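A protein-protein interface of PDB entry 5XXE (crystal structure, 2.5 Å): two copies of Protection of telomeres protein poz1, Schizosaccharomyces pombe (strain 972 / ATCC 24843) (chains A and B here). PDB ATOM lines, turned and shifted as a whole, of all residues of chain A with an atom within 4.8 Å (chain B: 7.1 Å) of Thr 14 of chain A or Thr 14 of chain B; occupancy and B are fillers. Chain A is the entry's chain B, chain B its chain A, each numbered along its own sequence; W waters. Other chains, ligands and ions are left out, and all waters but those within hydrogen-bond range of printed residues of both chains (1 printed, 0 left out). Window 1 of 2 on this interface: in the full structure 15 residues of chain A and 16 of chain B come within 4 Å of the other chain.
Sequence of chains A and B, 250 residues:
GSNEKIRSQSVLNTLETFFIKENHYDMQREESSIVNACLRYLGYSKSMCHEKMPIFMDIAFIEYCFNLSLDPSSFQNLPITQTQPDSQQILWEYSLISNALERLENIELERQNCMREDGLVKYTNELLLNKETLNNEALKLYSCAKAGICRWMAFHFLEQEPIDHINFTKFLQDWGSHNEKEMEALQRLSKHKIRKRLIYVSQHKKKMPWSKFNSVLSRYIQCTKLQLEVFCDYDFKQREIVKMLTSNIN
Ser 10 of chain A touches Thr 14 of chain B, and with the chains exchanged Thr 14 of chain A touches Ser 10 of chain B. Ser 10 of chain A touches Thr 17 of chain B, and with the chains exchanged Thr 17 of chain A touches Ser 10 of chain B. Val 11 of chain A touches Thr 14 of chain B, and with the chains exchanged Thr 14 of chain A touches Val 11 of chain B. Thr 14 of chain A touches its own counterpart, Thr 14 of chain B. Of the 14 pairs that touch across the chains among the printed residues, 11 have their exchanged pair printed and touching as well.
OG1 of Thr 14 of chain A is in hydrogen-bond range of OG of Ser 10 of chain B (2.9 Å). OG1 of Thr 14 of chain B is in hydrogen-bond range of OG1 of Thr 14 of chain A (2.7 Å). The backbone carbonyl oxygen of Ser 10 of chain A lies within hydrogen-bond range of the side-chain hydroxyl of Thr 14 of chain B, at 3.0 Å.
O of Thr 14 of chain B is in hydrogen-bond range of OG1 of Thr 17 of chain B (2.9 Å). The side-chain hydroxyl of Thr 17 of chain A lies within hydrogen-bond range of the backbone carbonyl oxygen of Asn 13 of chain A, 2.9 Å away. The side-chain hydroxyl of Thr 14 of chain A lies within hydrogen-bond range of the backbone carbonyl oxygen of Ser 10 of chain A (3.3 Å). The side-chain sulfur (SG) of Cys 38 of chain B sits at hydrogen-bond distance from the backbone carbonyl oxygen (O) of Ile 34 of chain B (3.2 Å). The side-chain amide nitrogen (ND2) of Asn 13 of chain B lies close to the backbone carbonyl oxygen (O) of Gln 9 of chain B (3.2 Å).
Asn 13 of chain B touches Ser 10 of chain A (O to OG, 3.7 Å). Ser 10 of chain A touches Thr 17 of chain B. Val 11 of chain A touches Thr 14 of chain B. Val 11 of chain A touches Phe 18 of chain B (CG2 to CE1, 3.9 Å). Val 11 of chain A touches Ile 34 of chain B (CG2 to CD1, 3.4 Å). OG of Ser 10 of chain B touches O of Asn 13 of chain A, 3.8 Å away. Val 11 of chain B touches Thr 14 of chain A (CG2 to CG2, 3.9 Å). Thr 17 of chain A touches Arg 7 of chain B (O to CG, 3.7 Å). Phe 18 of chain A touches Arg 7 of chain B. CG2 of Val 11 of chain B touches CE1 of Phe 18 of chain A, at 3.9 Å.
Water W1 lies within hydrogen-bond range of the backbone carbonyl oxygen of Arg 7 of chain B, the backbone carbonyl oxygen of Thr 14 of chain A and the side-chain hydroxyl of Ser 10 of chain B.
Of the 10 printed residues of chain A, 6 touch a printed residue of chain B. Printed residues of chain A that touch a printed residue of chain B: Ser 10, Val 11, Asn 13, Thr 14, Thr 17 and Phe 18. Of the 16 printed residues of chain B, 8 touch a printed residue of chain A. Printed residues of chain B that touch a printed residue of chain A: Arg 7, Ser 10, Val 11, Asn 13, Thr 14, Thr 17, Phe 18 and Ile 34. Hydrophobic or aromatic side chains of chain B within 4 Å of the printed part of chain A: Val 11, Phe 18 and Ile 34. Among the printed residues, 14 pairs touch across the chains. Among the printed residues, no Asp or Glu carboxylate lies within 4 Å of a Lys or Arg side-chain nitrogen of the other chain.
Of chain B, only Ser 10 (2.9 Å), Val 11 (3.9 Å) and Thr 14 (2.7 Å) come within 4 Å of Thr 14 of chain A. Thr 14 of chain B touches three residues of chain A. Of the printed residues of chain A, Thr 17 of chain B touches Ser 10. Of the printed residues of chain B, Phe 18 of chain A touches Arg 7 and Val 11. Of the printed residues of chain B, Asn 13 of chain A touches Ser 10 (3.8 Å). Printed residues of chain A within 4 Å of Val 11 of chain B: Thr 14 and Phe 18. The nearest residue of chain B that does not touch Thr 14 of chain A is Arg 7 of chain B (5.1 Å). The nearest printed residue of chain A that does not touch Val 11 of chain B is Ser 10 of chain A (6.6 Å).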
ATOM      1  N   SER A  10      19.331   8.200 -11.962  1.00  0.00           N
ATOM      2  CA  SER A  10      18.437   7.275 -12.657  1.00  0.00           C
ATOM      3  C   SER A  10      19.196   6.320 -13.596  1.00  0.00           C
ATOM      4  O   SER A  10      18.878   5.133 -13.670  1.00  0.00           O
ATOM      5  CB  SER A  10      17.361   8.043 -13.431  1.00  0.00           C
ATOM      6  OG  SER A  10      16.289   7.170 -13.769  1.00  0.00           O
ATOM      7  N   VAL A  11      20.192   6.845 -14.307  1.00  0.00           N
ATOM      8  CA  VAL A  11      21.080   6.027 -15.142  1.00  0.00           C
ATOM      9  C   VAL A  11      21.801   4.986 -14.278  1.00  0.00           C
ATOM     10  O   VAL A  11      21.942   3.820 -14.677  1.00  0.00           O
ATOM     11  CB  VAL A  11      22.109   6.900 -15.900  1.00  0.00           C
ATOM     12  CG1 VAL A  11      23.196   6.050 -16.548  1.00  0.00           C
ATOM     13  CG2 VAL A  11      21.411   7.737 -16.963  1.00  0.00           C
ATOM     14  N   LEU A  12      22.244   5.424 -13.100  1.00  0.00           N
ATOM     15  CA  LEU A  12      22.884   4.548 -12.122  1.00  0.00           C
ATOM     16  C   LEU A  12      21.939   3.466 -11.601  1.00  0.00           C
ATOM     17  O   LEU A  12      22.359   2.323 -11.461  1.00  0.00           O
ATOM     18  CB  LEU A  12      23.471   5.363 -10.967  1.00  0.00           C
ATOM     19  CG  LEU A  12      24.438   4.667 -10.011  1.00  0.00           C
ATOM     20  CD1 LEU A  12      25.629   4.057 -10.733  1.00  0.00           C
ATOM     21  CD2 LEU A  12      24.905   5.675  -8.971  1.00  0.00           C
ATOM     22  N   ASN A  13      20.671   3.803 -11.351  1.00  0.00           N
ATOM     23  CA  ASN A  13      19.667   2.788 -10.952  1.00  0.00           C
ATOM     24  C   ASN A  13      19.375   1.781 -12.049  1.00  0.00           C
ATOM     25  O   ASN A  13      19.064   0.634 -11.773  1.00  0.00           O
ATOM     26  CB  ASN A  13      18.338   3.418 -10.528  1.00  0.00           C
ATOM     27  CG  ASN A  13      18.457   4.282  -9.292  1.00  0.00           C
ATOM     28  OD1 ASN A  13      19.432   4.208  -8.540  1.00  0.00           O
ATOM     29  ND2 ASN A  13      17.456   5.137  -9.085  1.00  0.00           N
ATOM     30  N   THR A  14      19.433   2.220 -13.295  1.00  0.00           N
ATOM     31  CA  THR A  14      19.242   1.326 -14.434  1.00  0.00           C
ATOM     32  C   THR A  14      20.442   0.412 -14.578  1.00  0.00           C
ATOM     33  O   THR A  14      20.274  -0.759 -14.873  1.00  0.00           O
ATOM     34  CB  THR A  14      18.952   2.124 -15.730  1.00  0.00           C
ATOM     35  OG1 THR A  14      17.678   2.757 -15.605  1.00  0.00           O
ATOM     36  CG2 THR A  14      18.925   1.232 -16.961  1.00  0.00           C
ATOM     37  N   LEU A  15      21.645   0.943 -14.366  1.00  0.00           N
ATOM     38  CA  LEU A  15      22.846   0.100 -14.362  1.00  0.00           C
ATOM     39  C   LEU A  15      22.792  -0.965 -13.282  1.00  0.00           C
ATOM     40  O   LEU A  15      23.148  -2.100 -13.557  1.00  0.00           O
ATOM     41  CB  LEU A  15      24.132   0.914 -14.225  1.00  0.00           C
ATOM     42  CG  LEU A  15      24.754   1.379 -15.536  1.00  0.00           C
ATOM     43  CD1 LEU A  15      26.077   2.069 -15.236  1.00  0.00           C
ATOM     44  CD2 LEU A  15      24.960   0.236 -16.528  1.00  0.00           C
ATOM     45  N   GLU A  16      22.318  -0.598 -12.089  1.00  0.00           N
ATOM     46  CA  GLU A  16      22.129  -1.537 -10.972  1.00  0.00           C
ATOM     47  C   GLU A  16      21.302  -2.742 -11.363  1.00  0.00           C
ATOM     48  O   GLU A  16      21.630  -3.873 -11.024  1.00  0.00           O
ATOM     49  CB  GLU A  16      21.453  -0.839  -9.789  1.00  0.00           C
ATOM     50  CG  GLU A  16      21.573  -1.601  -8.475  1.00  0.00           C
ATOM     51  CD  GLU A  16      21.065  -0.820  -7.278  1.00  0.00           C
ATOM     52  OE1 GLU A  16      20.282   0.129  -7.469  1.00  0.00           O
ATOM     53  OE2 GLU A  16      21.435  -1.153  -6.130  1.00  0.00           O
ATOM     54  N   THR A  17      20.234  -2.474 -12.099  1.00  0.00           N
ATOM     55  CA  THR A  17      19.323  -3.492 -12.599  1.00  0.00           C
ATOM     56  C   THR A  17      19.925  -4.402 -13.693  1.00  0.00           C
ATOM     57  O   THR A  17      19.446  -5.517 -13.896  1.00  0.00           O
ATOM     58  CB  THR A  17      18.061  -2.791 -13.127  1.00  0.00           C
ATOM     59  OG1 THR A  17      17.619  -1.816 -12.175  1.00  0.00           O
ATOM     60  CG2 THR A  17      16.944  -3.745 -13.345  1.00  0.00           C
ATOM     61  N   PHE A  18      20.954  -3.931 -14.400  1.00  0.00           N
ATOM     62  CA  PHE A  18      21.666  -4.737 -15.421  1.00  0.00           C
ATOM     63  C   PHE A  18      22.888  -5.485 -14.875  1.00  0.00           C
ATOM     64  O   PHE A  18      23.277  -6.513 -15.430  1.00  0.00           O
ATOM     65  CB  PHE A  18      22.164  -3.841 -16.574  1.00  0.00           C
ATOM     66  CG  PHE A  18      21.134  -3.564 -17.638  1.00  0.00           C
ATOM     67  CD1 PHE A  18      20.073  -2.718 -17.394  1.00  0.00           C
ATOM     68  CD2 PHE A  18      21.254  -4.128 -18.895  1.00  0.00           C
ATOM     69  CE1 PHE A  18      19.131  -2.456 -18.371  1.00  0.00           C
ATOM     70  CE2 PHE A  18      20.325  -3.869 -19.881  1.00  0.00           C
ATOM     71  CZ  PHE A  18      19.256  -3.028 -19.617  1.00  0.00           C
ATOM     72  N   CYS A  38      24.967   4.145 -20.816  1.00  0.00           N
ATOM     73  CA  CYS A  38      24.885   4.493 -19.396  1.00  0.00           C
ATOM     74  C   CYS A  38      26.275   4.779 -18.796  1.00  0.00           C
ATOM     75  O   CYS A  38      26.440   5.770 -18.111  1.00  0.00           O
ATOM     76  CB  CYS A  38      24.186   3.393 -18.603  1.00  0.00           C
ATOM     77  SG  CYS A  38      22.434   3.169 -19.003  1.00  0.00           S
ATOM     78  N   ARG B   7      14.209  -4.775 -15.940  1.00  0.00           N
ATOM     79  CA  ARG B   7      15.183  -3.989 -16.696  1.00  0.00           C
ATOM     80  C   ARG B   7      14.489  -2.954 -17.571  1.00  0.00           C
ATOM     81  O   ARG B   7      14.822  -1.767 -17.514  1.00  0.00           O
ATOM     82  CB  ARG B   7      16.100  -4.879 -17.550  1.00  0.00           C
ATOM     83  CG  ARG B   7      17.140  -5.619 -16.726  1.00  0.00           C
ATOM     84  CD  ARG B   7      18.308  -6.113 -17.552  1.00  0.00           C
ATOM     85  NE  ARG B   7      17.923  -7.120 -18.527  1.00  0.00           N
ATOM     86  CZ  ARG B   7      17.613  -8.386 -18.247  1.00  0.00           C
ATOM     87  NH1 ARG B   7      17.611  -8.846 -16.999  1.00  0.00           N
ATOM     88  NH2 ARG B   7      17.282  -9.209 -19.240  1.00  0.00           N
ATOM     89  N   SER B   8      13.516  -3.413 -18.356  1.00  0.00           N
ATOM     90  CA  SER B   8      12.720  -2.536 -19.228  1.00  0.00           C
ATOM     91  C   SER B   8      11.959  -1.446 -18.476  1.00  0.00           C
ATOM     92  O   SER B   8      11.911  -0.312 -18.933  1.00  0.00           O
ATOM     93  CB  SER B   8      11.762  -3.356 -20.074  1.00  0.00           C
ATOM     94  OG  SER B   8      12.493  -4.081 -21.044  1.00  0.00           O
ATOM     95  N   GLN B   9      11.378  -1.786 -17.330  1.00  0.00           N
ATOM     96  CA  GLN B   9      10.719  -0.789 -16.475  1.00  0.00           C
ATOM     97  C   GLN B   9      11.700   0.274 -16.006  1.00  0.00           C
ATOM     98  O   GLN B   9      11.374   1.459 -15.962  1.00  0.00           O
ATOM     99  CB  GLN B   9      10.046  -1.442 -15.251  1.00  0.00           C
ATOM    100  CG  GLN B   9       8.631  -1.974 -15.501  1.00  0.00           C
ATOM    101  CD  GLN B   9       7.576  -0.881 -15.668  1.00  0.00           C
ATOM    102  OE1 GLN B   9       6.442  -1.170 -16.051  1.00  0.00           O
ATOM    103  NE2 GLN B   9       7.939   0.375 -15.384  1.00  0.00           N
ATOM    104  N   SER B  10      12.897  -0.163 -15.647  1.00  0.00           N
ATOM    105  CA  SER B  10      13.929   0.736 -15.163  1.00  0.00           C
ATOM    106  C   SER B  10      14.426   1.652 -16.279  1.00  0.00           C
ATOM    107  O   SER B  10      14.656   2.831 -16.043  1.00  0.00           O
ATOM    108  CB  SER B  10      15.081  -0.062 -14.554  1.00  0.00           C
ATOM    109  OG  SER B  10      16.096   0.803 -14.082  1.00  0.00           O
ATOM    110  N   VAL B  11      14.573   1.106 -17.488  1.00  0.00           N
ATOM    111  CA  VAL B  11      14.956   1.883 -18.672  1.00  0.00           C
ATOM    112  C   VAL B  11      13.900   2.952 -18.974  1.00  0.00           C
ATOM    113  O   VAL B  11      14.233   4.100 -19.268  1.00  0.00           O
ATOM    114  CB  VAL B  11      15.172   0.960 -19.891  1.00  0.00           C
ATOM    115  CG1 VAL B  11      15.295   1.754 -21.193  1.00  0.00           C
ATOM    116  CG2 VAL B  11      16.418   0.097 -19.684  1.00  0.00           C
ATOM    117  N   LEU B  12      12.632   2.567 -18.875  1.00  0.00           N
ATOM    118  CA  LEU B  12      11.514   3.499 -19.005  1.00  0.00           C
ATOM    119  C   LEU B  12      11.523   4.609 -17.943  1.00  0.00           C
ATOM    120  O   LEU B  12      11.261   5.771 -18.262  1.00  0.00           O
ATOM    121  CB  LEU B  12      10.186   2.729 -18.965  1.00  0.00           C
ATOM    122  CG  LEU B  12       8.877   3.496 -19.151  1.00  0.00           C
ATOM    123  CD1 LEU B  12       8.928   4.333 -20.410  1.00  0.00           C
ATOM    124  CD2 LEU B  12       7.723   2.513 -19.207  1.00  0.00           C
ATOM    125  N   ASN B  13      11.847   4.261 -16.697  1.00  0.00           N
ATOM    126  CA  ASN B  13      11.962   5.259 -15.623  1.00  0.00           C
ATOM    127  C   ASN B  13      13.096   6.243 -15.879  1.00  0.00           C
ATOM    128  O   ASN B  13      12.995   7.410 -15.504  1.00  0.00           O
ATOM    129  CB  ASN B  13      12.138   4.598 -14.245  1.00  0.00           C
ATOM    130  CG  ASN B  13      10.930   3.765 -13.827  1.00  0.00           C
ATOM    131  OD1 ASN B  13       9.800   4.027 -14.240  1.00  0.00           O
ATOM    132  ND2 ASN B  13      11.170   2.745 -13.018  1.00  0.00           N
ATOM    133  N   THR B  14      14.173   5.785 -16.514  1.00  0.00           N
ATOM    134  CA  THR B  14      15.264   6.688 -16.889  1.00  0.00           C
ATOM    135  C   THR B  14      14.813   7.642 -17.996  1.00  0.00           C
ATOM    136  O   THR B  14      15.107   8.830 -17.921  1.00  0.00           O
ATOM    137  CB  THR B  14      16.570   5.929 -17.238  1.00  0.00           C
ATOM    138  OG1 THR B  14      17.106   5.367 -16.038  1.00  0.00           O
ATOM    139  CG2 THR B  14      17.637   6.856 -17.831  1.00  0.00           C
ATOM    140  N   LEU B  15      14.084   7.137 -18.994  1.00  0.00           N
ATOM    141  CA  LEU B  15      13.519   8.013 -20.036  1.00  0.00           C
ATOM    142  C   LEU B  15      12.624   9.093 -19.437  1.00  0.00           C
ATOM    143  O   LEU B  15      12.691  10.242 -19.854  1.00  0.00           O
ATOM    144  CB  LEU B  15      12.747   7.232 -21.110  1.00  0.00           C
ATOM    145  CG  LEU B  15      13.565   6.664 -22.269  1.00  0.00           C
ATOM    146  CD1 LEU B  15      12.661   5.893 -23.219  1.00  0.00           C
ATOM    147  CD2 LEU B  15      14.320   7.755 -23.015  1.00  0.00           C
ATOM    148  N   GLU B  16      11.825   8.728 -18.442  1.00  0.00           N
ATOM    149  CA  GLU B  16      10.968   9.691 -17.754  1.00  0.00           C
ATOM    150  C   GLU B  16      11.732  10.894 -17.186  1.00  0.00           C
ATOM    151  O   GLU B  16      11.244  12.014 -17.278  1.00  0.00           O
ATOM    152  CB  GLU B  16      10.155   9.006 -16.648  1.00  0.00           C
ATOM    153  CG  GLU B  16       8.927   9.798 -16.234  1.00  0.00           C
ATOM    154  CD  GLU B  16       8.126   9.140 -15.128  1.00  0.00           C
ATOM    155  OE1 GLU B  16       7.978   7.901 -15.132  1.00  0.00           O
ATOM    156  OE2 GLU B  16       7.619   9.877 -14.256  1.00  0.00           O
ATOM    157  N   THR B  17      12.926  10.669 -16.633  1.00  0.00           N
ATOM    158  CA  THR B  17      13.758  11.767 -16.097  1.00  0.00           C
ATOM    159  C   THR B  17      14.418  12.594 -17.201  1.00  0.00           C
ATOM    160  O   THR B  17      14.700  13.769 -17.002  1.00  0.00           O
ATOM    161  CB  THR B  17      14.877  11.283 -15.141  1.00  0.00           C
ATOM    162  OG1 THR B  17      15.955  10.697 -15.895  1.00  0.00           O
ATOM    163  CG2 THR B  17      14.348  10.283 -14.118  1.00  0.00           C
ATOM    164  N   PHE B  18      14.707  11.972 -18.339  1.00  0.00           N
ATOM    165  CA  PHE B  18      15.243  12.700 -19.499  1.00  0.00           C
ATOM    166  C   PHE B  18      14.177  13.488 -20.285  1.00  0.00           C
ATOM    167  O   PHE B  18      14.500  14.537 -20.832  1.00  0.00           O
ATOM    168  CB  PHE B  18      15.978  11.749 -20.460  1.00  0.00           C
ATOM    169  CG  PHE B  18      17.389  11.451 -20.060  1.00  0.00           C
ATOM    170  CD1 PHE B  18      17.660  10.567 -19.022  1.00  0.00           C
ATOM    171  CD2 PHE B  18      18.454  12.045 -20.720  1.00  0.00           C
ATOM    172  CE1 PHE B  18      18.965  10.283 -18.646  1.00  0.00           C
ATOM    173  CE2 PHE B  18      19.766  11.764 -20.353  1.00  0.00           C
ATOM    174  CZ  PHE B  18      20.019  10.879 -19.315  1.00  0.00           C
ATOM    175  N   PHE B  19      12.937  12.981 -20.335  1.00  0.00           N
ATOM    176  CA  PHE B  19      11.879  13.503 -21.224  1.00  0.00           C
ATOM    177  C   PHE B  19      10.957  14.545 -20.593  1.00  0.00           C
ATOM    178  O   PHE B  19      10.628  15.540 -21.234  1.00  0.00           O
ATOM    179  CB  PHE B  19      10.998  12.366 -21.757  1.00  0.00           C
ATOM    180  CG  PHE B  19      11.582  11.595 -22.910  1.00  0.00           C
ATOM    181  CD1 PHE B  19      12.784  11.942 -23.522  1.00  0.00           C
ATOM    182  CD2 PHE B  19      10.873  10.521 -23.421  1.00  0.00           C
ATOM    183  CE1 PHE B  19      13.269  11.215 -24.593  1.00  0.00           C
ATOM    184  CE2 PHE B  19      11.352   9.792 -24.495  1.00  0.00           C
ATOM    185  CZ  PHE B  19      12.555  10.140 -25.084  1.00  0.00           C
ATOM    186  N   ILE B  34      22.252   7.957 -25.122  1.00  0.00           N
ATOM    187  CA  ILE B  34      21.526   7.208 -24.095  1.00  0.00           C
ATOM    188  C   ILE B  34      20.021   7.121 -24.373  1.00  0.00           C
ATOM    189  O   ILE B  34      19.412   6.064 -24.178  1.00  0.00           O
ATOM    190  CB  ILE B  34      21.816   7.741 -22.666  1.00  0.00           C
ATOM    191  CG1 ILE B  34      21.371   6.721 -21.615  1.00  0.00           C
ATOM    192  CG2 ILE B  34      21.166   9.095 -22.404  1.00  0.00           C
ATOM    193  CD1 ILE B  34      21.874   7.043 -20.232  1.00  0.00           C
ATOM    194  N   CYS B  38      18.047   3.795 -24.903  1.00  0.00           N
ATOM    195  CA  CYS B  38      16.829   3.495 -24.137  1.00  0.00           C
ATOM    196  C   CYS B  38      15.625   3.168 -25.046  1.00  0.00           C
ATOM    197  O   CYS B  38      14.892   2.203 -24.790  1.00  0.00           O
ATOM    198  CB  CYS B  38      16.464   4.657 -23.191  1.00  0.00           C
ATOM    199  SG  CYS B  38      17.576   4.915 -21.785  1.00  0.00           S
ATOM    200  N   PHE B  56       3.773  10.507 -21.053  1.00  0.00           N
ATOM    201  CA  PHE B  56       4.992  11.322 -21.214  1.00  0.00           C
ATOM    202  C   PHE B  56       5.805  10.949 -22.459  1.00  0.00           C
ATOM    203  O   PHE B  56       6.572  11.770 -22.948  1.00  0.00           O
ATOM    204  CB  PHE B  56       5.888  11.282 -19.955  1.00  0.00           C
ATOM    205  CG  PHE B  56       6.828  10.098 -19.888  1.00  0.00           C
ATOM    206  CD1 PHE B  56       8.068  10.130 -20.533  1.00  0.00           C
ATOM    207  CD2 PHE B  56       6.492   8.961 -19.158  1.00  0.00           C
ATOM    208  CE1 PHE B  56       8.928   9.041 -20.479  1.00  0.00           C
ATOM    209  CE2 PHE B  56       7.356   7.875 -19.092  1.00  0.00           C
ATOM    210  CZ  PHE B  56       8.574   7.915 -19.751  1.00  0.00           C
HETATM  211  O   HOH W   1      17.480  -1.705 -15.946  1.00  0.00           O
